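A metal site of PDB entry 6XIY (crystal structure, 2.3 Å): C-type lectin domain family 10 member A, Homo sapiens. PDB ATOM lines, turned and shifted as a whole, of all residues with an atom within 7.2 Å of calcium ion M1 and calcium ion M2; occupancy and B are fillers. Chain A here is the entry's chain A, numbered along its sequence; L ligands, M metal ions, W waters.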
ATOM      1  N   SER A  63      29.309   5.252  -0.079  1.00  0.00           N
ATOM      2  CA  SER A  63      28.112   4.612   0.513  1.00  0.00           C
ATOM      3  C   SER A  63      28.507   3.837   1.783  1.00  0.00           C
ATOM      4  O   SER A  63      29.706   3.574   1.948  1.00  0.00           O
ATOM      5  CB  SER A  63      27.406   3.742  -0.508  1.00  0.00           C
ATOM      6  OG  SER A  63      28.262   2.707  -0.975  1.00  0.00           O
ATOM      7  N   ASP A  64      27.543   3.591   2.678  1.00  0.00           N
ATOM      8  CA  ASP A  64      27.750   2.880   3.975  1.00  0.00           C
ATOM      9  C   ASP A  64      26.594   1.917   4.234  1.00  0.00           C
ATOM     10  O   ASP A  64      26.141   1.832   5.370  1.00  0.00           O
ATOM     11  CB  ASP A  64      27.900   3.868   5.146  1.00  0.00           C
ATOM     12  CG  ASP A  64      26.636   4.560   5.631  1.00  0.00           C
ATOM     13  OD1 ASP A  64      25.653   4.671   4.861  1.00  0.00           O
ATOM     14  OD2 ASP A  64      26.585   5.012   6.793  1.00  0.00           O
ATOM     15  N   PRO A  65      26.099   1.142   3.244  1.00  0.00           N
ATOM     16  CA  PRO A  65      24.943   0.265   3.475  1.00  0.00           C
ATOM     17  C   PRO A  65      25.270  -0.809   4.531  1.00  0.00           C
ATOM     18  O   PRO A  65      24.409  -1.120   5.342  1.00  0.00           O
ATOM     19  CB  PRO A  65      24.631  -0.353   2.096  1.00  0.00           C
ATOM     20  CG  PRO A  65      25.936  -0.224   1.337  1.00  0.00           C
ATOM     21  CD  PRO A  65      26.585   1.044   1.861  1.00  0.00           C
ATOM     22  N   GLY A  67      27.317  -0.436   7.141  1.00  0.00           N
ATOM     23  CA  GLY A  67      27.695   0.162   8.449  1.00  0.00           C
ATOM     24  C   GLY A  67      28.865   1.139   8.382  1.00  0.00           C
ATOM     25  O   GLY A  67      28.798   2.145   9.119  1.00  0.00           O
ATOM     26  N   TRP A  69      31.561   3.655   5.937  1.00  0.00           N
ATOM     27  CA  TRP A  69      31.690   4.407   4.655  1.00  0.00           C
ATOM     28  C   TRP A  69      32.758   3.784   3.755  1.00  0.00           C
ATOM     29  O   TRP A  69      33.834   3.517   4.260  1.00  0.00           O
ATOM     30  CB  TRP A  69      31.966   5.882   4.896  1.00  0.00           C
ATOM     31  CG  TRP A  69      30.747   6.584   5.385  1.00  0.00           C
ATOM     32  CD1 TRP A  69      30.429   6.893   6.673  1.00  0.00           C
ATOM     33  CD2 TRP A  69      29.633   6.992   4.574  1.00  0.00           C
ATOM     34  NE1 TRP A  69      29.207   7.502   6.710  1.00  0.00           N
ATOM     35  CE2 TRP A  69      28.683   7.560   5.444  1.00  0.00           C
ATOM     36  CE3 TRP A  69      29.338   6.905   3.209  1.00  0.00           C
ATOM     37  CZ2 TRP A  69      27.469   8.056   4.989  1.00  0.00           C
ATOM     38  CZ3 TRP A  69      28.137   7.408   2.771  1.00  0.00           C
ATOM     39  CH2 TRP A  69      27.214   7.970   3.646  1.00  0.00           C
ATOM     40  N   TRP A  84      32.272  16.954   4.275  1.00  0.00           N
ATOM     41  CA  TRP A  84      30.860  16.873   4.722  1.00  0.00           C
ATOM     42  C   TRP A  84      30.338  18.254   5.087  1.00  0.00           C
ATOM     43  O   TRP A  84      31.131  19.085   5.625  1.00  0.00           O
ATOM     44  CB  TRP A  84      30.704  15.932   5.897  1.00  0.00           C
ATOM     45  CG  TRP A  84      31.029  14.505   5.608  1.00  0.00           C
ATOM     46  CD1 TRP A  84      32.164  13.875   5.981  1.00  0.00           C
ATOM     47  CD2 TRP A  84      30.219  13.522   4.949  1.00  0.00           C
ATOM     48  NE1 TRP A  84      32.123  12.575   5.588  1.00  0.00           N
ATOM     49  CE2 TRP A  84      30.939  12.316   4.967  1.00  0.00           C
ATOM     50  CE3 TRP A  84      28.966  13.535   4.325  1.00  0.00           C
ATOM     51  CZ2 TRP A  84      30.461  11.142   4.407  1.00  0.00           C
ATOM     52  CZ3 TRP A  84      28.473  12.373   3.777  1.00  0.00           C
ATOM     53  CH2 TRP A  84      29.213  11.186   3.832  1.00  0.00           C
ATOM     54  N   GLY A  87      27.002  18.880  10.336  1.00  0.00           N
ATOM     55  CA  GLY A  87      25.979  17.964  10.867  1.00  0.00           C
ATOM     56  C   GLY A  87      25.921  16.642  10.107  1.00  0.00           C
ATOM     57  O   GLY A  87      25.233  15.736  10.571  1.00  0.00           O
ATOM     58  N   GLN A  88      26.628  16.509   8.981  1.00  0.00           N
ATOM     59  CA  GLN A  88      26.626  15.272   8.163  1.00  0.00           C
ATOM     60  C   GLN A  88      27.941  14.530   8.370  1.00  0.00           C
ATOM     61  O   GLN A  88      28.962  15.136   8.715  1.00  0.00           O
ATOM     62  CB  GLN A  88      26.274  15.634   6.709  1.00  0.00           C
ATOM     63  CG  GLN A  88      25.060  16.552   6.588  1.00  0.00           C
ATOM     64  CD  GLN A  88      23.736  15.887   6.943  1.00  0.00           C
ATOM     65  OE1 GLN A  88      23.644  14.666   7.085  1.00  0.00           O
ATOM     66  NE2 GLN A  88      22.669  16.684   7.029  1.00  0.00           N
ATOM     67  N   PRO A  89      27.971  13.188   8.203  1.00  0.00           N
ATOM     68  CA  PRO A  89      26.773  12.409   7.880  1.00  0.00           C
ATOM     69  C   PRO A  89      25.940  12.143   9.150  1.00  0.00           C
ATOM     70  O   PRO A  89      26.519  12.213  10.195  1.00  0.00           O
ATOM     71  CB  PRO A  89      27.366  11.128   7.297  1.00  0.00           C
ATOM     72  CG  PRO A  89      28.717  10.957   7.975  1.00  0.00           C
ATOM     73  CD  PRO A  89      29.170  12.358   8.341  1.00  0.00           C
ATOM     74  N   ASP A  90      24.626  11.936   9.031  1.00  0.00           N
ATOM     75  CA  ASP A  90      23.702  11.831  10.206  1.00  0.00           C
ATOM     76  C   ASP A  90      22.837  10.557  10.145  1.00  0.00           C
ATOM     77  O   ASP A  90      22.072  10.364  11.093  1.00  0.00           O
ATOM     78  CB  ASP A  90      22.777  13.045  10.331  1.00  0.00           C
ATOM     79  CG  ASP A  90      21.884  13.306   9.111  1.00  0.00           C
ATOM     80  OD1 ASP A  90      22.031  12.608   8.039  1.00  0.00           O
ATOM     81  OD2 ASP A  90      21.046  14.225   9.234  1.00  0.00           O
ATOM     82  N   ASP A  91      22.880   9.795   9.051  1.00  0.00           N
ATOM     83  CA  ASP A  91      22.034   8.593   8.824  1.00  0.00           C
ATOM     84  C   ASP A  91      20.554   8.881   9.200  1.00  0.00           C
ATOM     85  O   ASP A  91      19.911   8.008   9.827  1.00  0.00           O
ATOM     86  CB  ASP A  91      22.618   7.415   9.615  1.00  0.00           C
ATOM     87  CG  ASP A  91      22.130   6.041   9.139  1.00  0.00           C
ATOM     88  OD1 ASP A  91      22.193   5.765   7.893  1.00  0.00           O
ATOM     89  OD2 ASP A  91      21.739   5.251  10.018  1.00  0.00           O
ATOM     90  N   TRP A  92      20.014  10.056   8.851  1.00  0.00           N
ATOM     91  CA  TRP A  92      18.642  10.531   9.241  1.00  0.00           C
ATOM     92  C   TRP A  92      17.582   9.494   8.877  1.00  0.00           C
ATOM     93  O   TRP A  92      17.709   8.920   7.768  1.00  0.00           O
ATOM     94  CB  TRP A  92      18.350  11.833   8.516  1.00  0.00           C
ATOM     95  CG  TRP A  92      17.156  12.602   8.975  1.00  0.00           C
ATOM     96  CD1 TRP A  92      16.834  12.923  10.256  1.00  0.00           C
ATOM     97  CD2 TRP A  92      16.181  13.244   8.139  1.00  0.00           C
ATOM     98  NE1 TRP A  92      15.697  13.683  10.273  1.00  0.00           N
ATOM     99  CE2 TRP A  92      15.275  13.906   8.986  1.00  0.00           C
ATOM    100  CE3 TRP A  92      15.964  13.316   6.756  1.00  0.00           C
ATOM    101  CZ2 TRP A  92      14.176  14.631   8.508  1.00  0.00           C
ATOM    102  CZ3 TRP A  92      14.889  14.048   6.276  1.00  0.00           C
ATOM    103  CH2 TRP A  92      14.005  14.695   7.145  1.00  0.00           C
ATOM    104  N   GLY A 100      17.944   4.545   7.197  1.00  0.00           N
ATOM    105  CA  GLY A 100      18.597   5.851   7.388  1.00  0.00           C
ATOM    106  C   GLY A 100      18.950   6.471   6.046  1.00  0.00           C
ATOM    107  O   GLY A 100      18.043   6.628   5.181  1.00  0.00           O
ATOM    108  N   GLU A 101      20.217   6.811   5.864  1.00  0.00           N
ATOM    109  CA  GLU A 101      20.778   7.446   4.650  1.00  0.00           C
ATOM    110  C   GLU A 101      22.147   6.805   4.386  1.00  0.00           C
ATOM    111  O   GLU A 101      22.980   6.827   5.293  1.00  0.00           O
ATOM    112  CB  GLU A 101      20.857   8.967   4.862  1.00  0.00           C
ATOM    113  CG  GLU A 101      19.498   9.644   5.020  1.00  0.00           C
ATOM    114  CD  GLU A 101      19.605  11.151   5.175  1.00  0.00           C
ATOM    115  OE1 GLU A 101      20.609  11.577   5.805  1.00  0.00           O
ATOM    116  OE2 GLU A 101      18.713  11.911   4.642  1.00  0.00           O
ATOM    117  N   ASP A 102      22.332   6.186   3.226  1.00  0.00           N
ATOM    118  CA  ASP A 102      23.471   5.281   2.972  1.00  0.00           C
ATOM    119  C   ASP A 102      24.244   5.665   1.718  1.00  0.00           C
ATOM    120  O   ASP A 102      25.153   4.924   1.380  1.00  0.00           O
ATOM    121  CB  ASP A 102      22.980   3.832   2.869  1.00  0.00           C
ATOM    122  CG  ASP A 102      22.444   3.355   4.208  1.00  0.00           C
ATOM    123  OD1 ASP A 102      22.717   4.064   5.269  1.00  0.00           O
ATOM    124  OD2 ASP A 102      21.747   2.315   4.210  1.00  0.00           O
ATOM    125  N   CYS A 103      23.940   6.811   1.100  1.00  0.00           N
ATOM    126  CA  CYS A 103      24.548   7.265  -0.175  1.00  0.00           C
ATOM    127  C   CYS A 103      24.872   8.759  -0.061  1.00  0.00           C
ATOM    128  O   CYS A 103      24.036   9.490   0.485  1.00  0.00           O
ATOM    129  CB  CYS A 103      23.596   6.992  -1.332  1.00  0.00           C
ATOM    130  SG  CYS A 103      23.422   5.228  -1.705  1.00  0.00           S
ATOM    131  N   HIS A 105      26.112  12.545  -1.619  1.00  0.00           N
ATOM    132  CA  HIS A 105      25.975  13.400  -2.807  1.00  0.00           C
ATOM    133  C   HIS A 105      26.601  14.735  -2.508  1.00  0.00           C
ATOM    134  O   HIS A 105      26.665  15.107  -1.341  1.00  0.00           O
ATOM    135  CB  HIS A 105      24.495  13.536  -3.194  1.00  0.00           C
ATOM    136  CG  HIS A 105      23.676  14.299  -2.221  1.00  0.00           C
ATOM    137  ND1 HIS A 105      23.464  15.663  -2.340  1.00  0.00           N
ATOM    138  CD2 HIS A 105      22.979  13.903  -1.135  1.00  0.00           C
ATOM    139  CE1 HIS A 105      22.682  16.072  -1.353  1.00  0.00           C
ATOM    140  NE2 HIS A 105      22.360  15.007  -0.608  1.00  0.00           N
ATOM    141  N   TRP A 112      29.286  17.658   1.178  1.00  0.00           N
ATOM    142  CA  TRP A 112      28.654  16.326   1.049  1.00  0.00           C
ATOM    143  C   TRP A 112      27.533  16.158   2.064  1.00  0.00           C
ATOM    144  O   TRP A 112      27.643  16.666   3.203  1.00  0.00           O
ATOM    145  CB  TRP A 112      29.696  15.236   1.205  1.00  0.00           C
ATOM    146  CG  TRP A 112      30.940  15.334   0.382  1.00  0.00           C
ATOM    147  CD1 TRP A 112      31.205  16.149  -0.677  1.00  0.00           C
ATOM    148  CD2 TRP A 112      32.092  14.501   0.539  1.00  0.00           C
ATOM    149  NE1 TRP A 112      32.469  15.899  -1.158  1.00  0.00           N
ATOM    150  CE2 TRP A 112      33.024  14.885  -0.435  1.00  0.00           C
ATOM    151  CE3 TRP A 112      32.420  13.473   1.424  1.00  0.00           C
ATOM    152  CZ2 TRP A 112      34.264  14.272  -0.549  1.00  0.00           C
ATOM    153  CZ3 TRP A 112      33.644  12.837   1.295  1.00  0.00           C
ATOM    154  CH2 TRP A 112      34.558  13.257   0.333  1.00  0.00           C
ATOM    155  N   ASN A 113      26.492  15.418   1.675  1.00  0.00           N
ATOM    156  CA  ASN A 113      25.400  14.976   2.580  1.00  0.00           C
ATOM    157  C   ASN A 113      25.162  13.479   2.339  1.00  0.00           C
ATOM    158  O   ASN A 113      25.390  13.029   1.212  1.00  0.00           O
ATOM    159  CB  ASN A 113      24.130  15.805   2.379  1.00  0.00           C
ATOM    160  CG  ASN A 113      22.935  15.201   3.091  1.00  0.00           C
ATOM    161  OD1 ASN A 113      22.990  14.941   4.299  1.00  0.00           O
ATOM    162  ND2 ASN A 113      21.877  14.918   2.345  1.00  0.00           N
ATOM    163  N   ASP A 114      24.743  12.734   3.356  1.00  0.00           N
ATOM    164  CA  ASP A 114      24.193  11.365   3.173  1.00  0.00           C
ATOM    165  C   ASP A 114      22.667  11.456   3.014  1.00  0.00           C
ATOM    166  O   ASP A 114      22.025  12.300   3.720  1.00  0.00           O
ATOM    167  CB  ASP A 114      24.583  10.422   4.318  1.00  0.00           C
ATOM    168  CG  ASP A 114      24.146  10.845   5.708  1.00  0.00           C
ATOM    169  OD1 ASP A 114      23.871  12.086   5.912  1.00  0.00           O
ATOM    170  OD2 ASP A 114      24.104   9.950   6.604  1.00  0.00           O
ATOM    171  N   ASP A 115      22.157  10.701   2.052  1.00  0.00           N
ATOM    172  CA  ASP A 115      20.742  10.748   1.606  1.00  0.00           C
ATOM    173  C   ASP A 115      20.326   9.329   1.219  1.00  0.00           C
ATOM    174  O   ASP A 115      21.195   8.388   1.230  1.00  0.00           O
ATOM    175  CB  ASP A 115      20.517  11.743   0.460  1.00  0.00           C
ATOM    176  CG  ASP A 115      19.179  12.506   0.505  1.00  0.00           C
ATOM    177  OD1 ASP A 115      18.180  11.924   0.983  1.00  0.00           O
ATOM    178  OD2 ASP A 115      19.151  13.683   0.063  1.00  0.00           O
ATOM    179  N   VAL A 116      19.041   9.223   0.905  1.00  0.00           N
ATOM    180  CA  VAL A 116      18.324   7.973   0.554  1.00  0.00           C
ATOM    181  C   VAL A 116      18.743   7.622  -0.863  1.00  0.00           C
ATOM    182  O   VAL A 116      18.572   8.476  -1.755  1.00  0.00           O
ATOM    183  CB  VAL A 116      16.802   8.187   0.691  1.00  0.00           C
ATOM    184  CG1 VAL A 116      16.011   6.949   0.269  1.00  0.00           C
ATOM    185  CG2 VAL A 116      16.444   8.598   2.118  1.00  0.00           C
HETATM  186  C1  LIG L   1      15.887  18.812   5.681  1.00  0.00           C
HETATM  187  S1  LIG L   1      16.879  17.626   4.702  1.00  0.00           S
HETATM  188  C2  LIG L   1      18.685  17.670   5.144  1.00  0.00           C
HETATM  189  C3  LIG L   1      18.940  17.625   6.641  1.00  0.00           C
HETATM  190  C4  LIG L   1      18.450  16.273   7.174  1.00  0.00           C
HETATM  191  C5  LIG L   1      18.567  16.272   8.724  1.00  0.00           C
HETATM  192  O1  LIG L   1      17.742  17.311   9.224  1.00  0.00           O
HETATM  193  C6  LIG L   1      19.160  15.060   6.539  1.00  0.00           C
HETATM  194  O2  LIG L   1      20.545  14.896   6.844  1.00  0.00           O
HETATM  195  C7  LIG L   1      19.125  15.080   5.009  1.00  0.00           C
HETATM  196  O3  LIG L   1      20.095  14.119   4.605  1.00  0.00           O
HETATM  197  C8  LIG L   1      19.467  16.481   4.495  1.00  0.00           C
HETATM  198  N1  LIG L   1      19.119  16.572   3.086  1.00  0.00           N
HETATM  199  C9  LIG L   1      19.973  17.320   2.183  1.00  0.00           C
HETATM  200  C10 LIG L   1      19.550  17.354   0.717  1.00  0.00           C
HETATM  201  O4  LIG L   1      20.988  17.820   2.567  1.00  0.00           O
HETATM  202 CA    CA M   1      24.182   5.339   6.654  1.00  0.00          CA
HETATM  203 CA    CA M   2      22.029  13.425   5.813  1.00  0.00          CA
HETATM  204  O   HOH W   1      24.858   7.498   7.296  1.00  0.00           O
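O of Glu 101 is bound to calcium ion M1 (2.3 Å).
Calcium ion M1 is bound by water W1 (2.4 Å).
Calcium ion M1 is bound by OD1 of Asp 91, 2.4 Å away.
OD1 of Asp 102 is bound to calcium ion M1 (2.4 Å).
OD1 of Asp 64 binds calcium ion M1 (2.4 Å).
OD2 of Asp 64 is bound to calcium ion M1.
The backbone NH (N) of Asp 91 is in hydrogen-bond range of the side-chain carboxylate (OD2) of Asp 114 (2.7 Å).
The side-chain carboxylate (OE1) of Glu 101 lies close to the backbone NH (N) of Trp 92.
The backbone carbonyl oxygen of Asn 113 is in hydrogen-bond range of the backbone NH of His 105.
The side-chain carboxylate (OD1) of Asp 90 sits close to the backbone NH (N) of Trp 92 (3.4 Å).
O of Asp 115 sits at hydrogen-bond distance from N of Asp 102, at 3.2 Å.
Of the 22 residues printed, 4 come within 4 Å of calcium ion M1.
Within 4 Å of calcium ion M2: Gln 88, Asp 90, Glu 101, Asn 113 and Asp 114.
The nearest printed residue that does not touch calcium ion M2 is Asp 115 (4.6 Å).
OD1 of Asp 114 binds calcium ion M2 (2.3 Å).
An oxygen (O2) of the ligand binds calcium ion M2.
OE1 of Glu 101 is bound to calcium ion M2, 2.3 Å away.
Calcium ion M2 is bound by OD1 of Asn 113, 2.3 Å away.
OD1 of Asp 90 binds calcium ion M2, at 2.4 Å.
O of Asp 114 is bound to calcium ion M2, at 2.4 Å.
An oxygen (O3) of the ligand binds calcium ion M2 (2.4 Å).
OE1 of Gln 88 is bound to calcium ion M2, 2.4 Å away.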
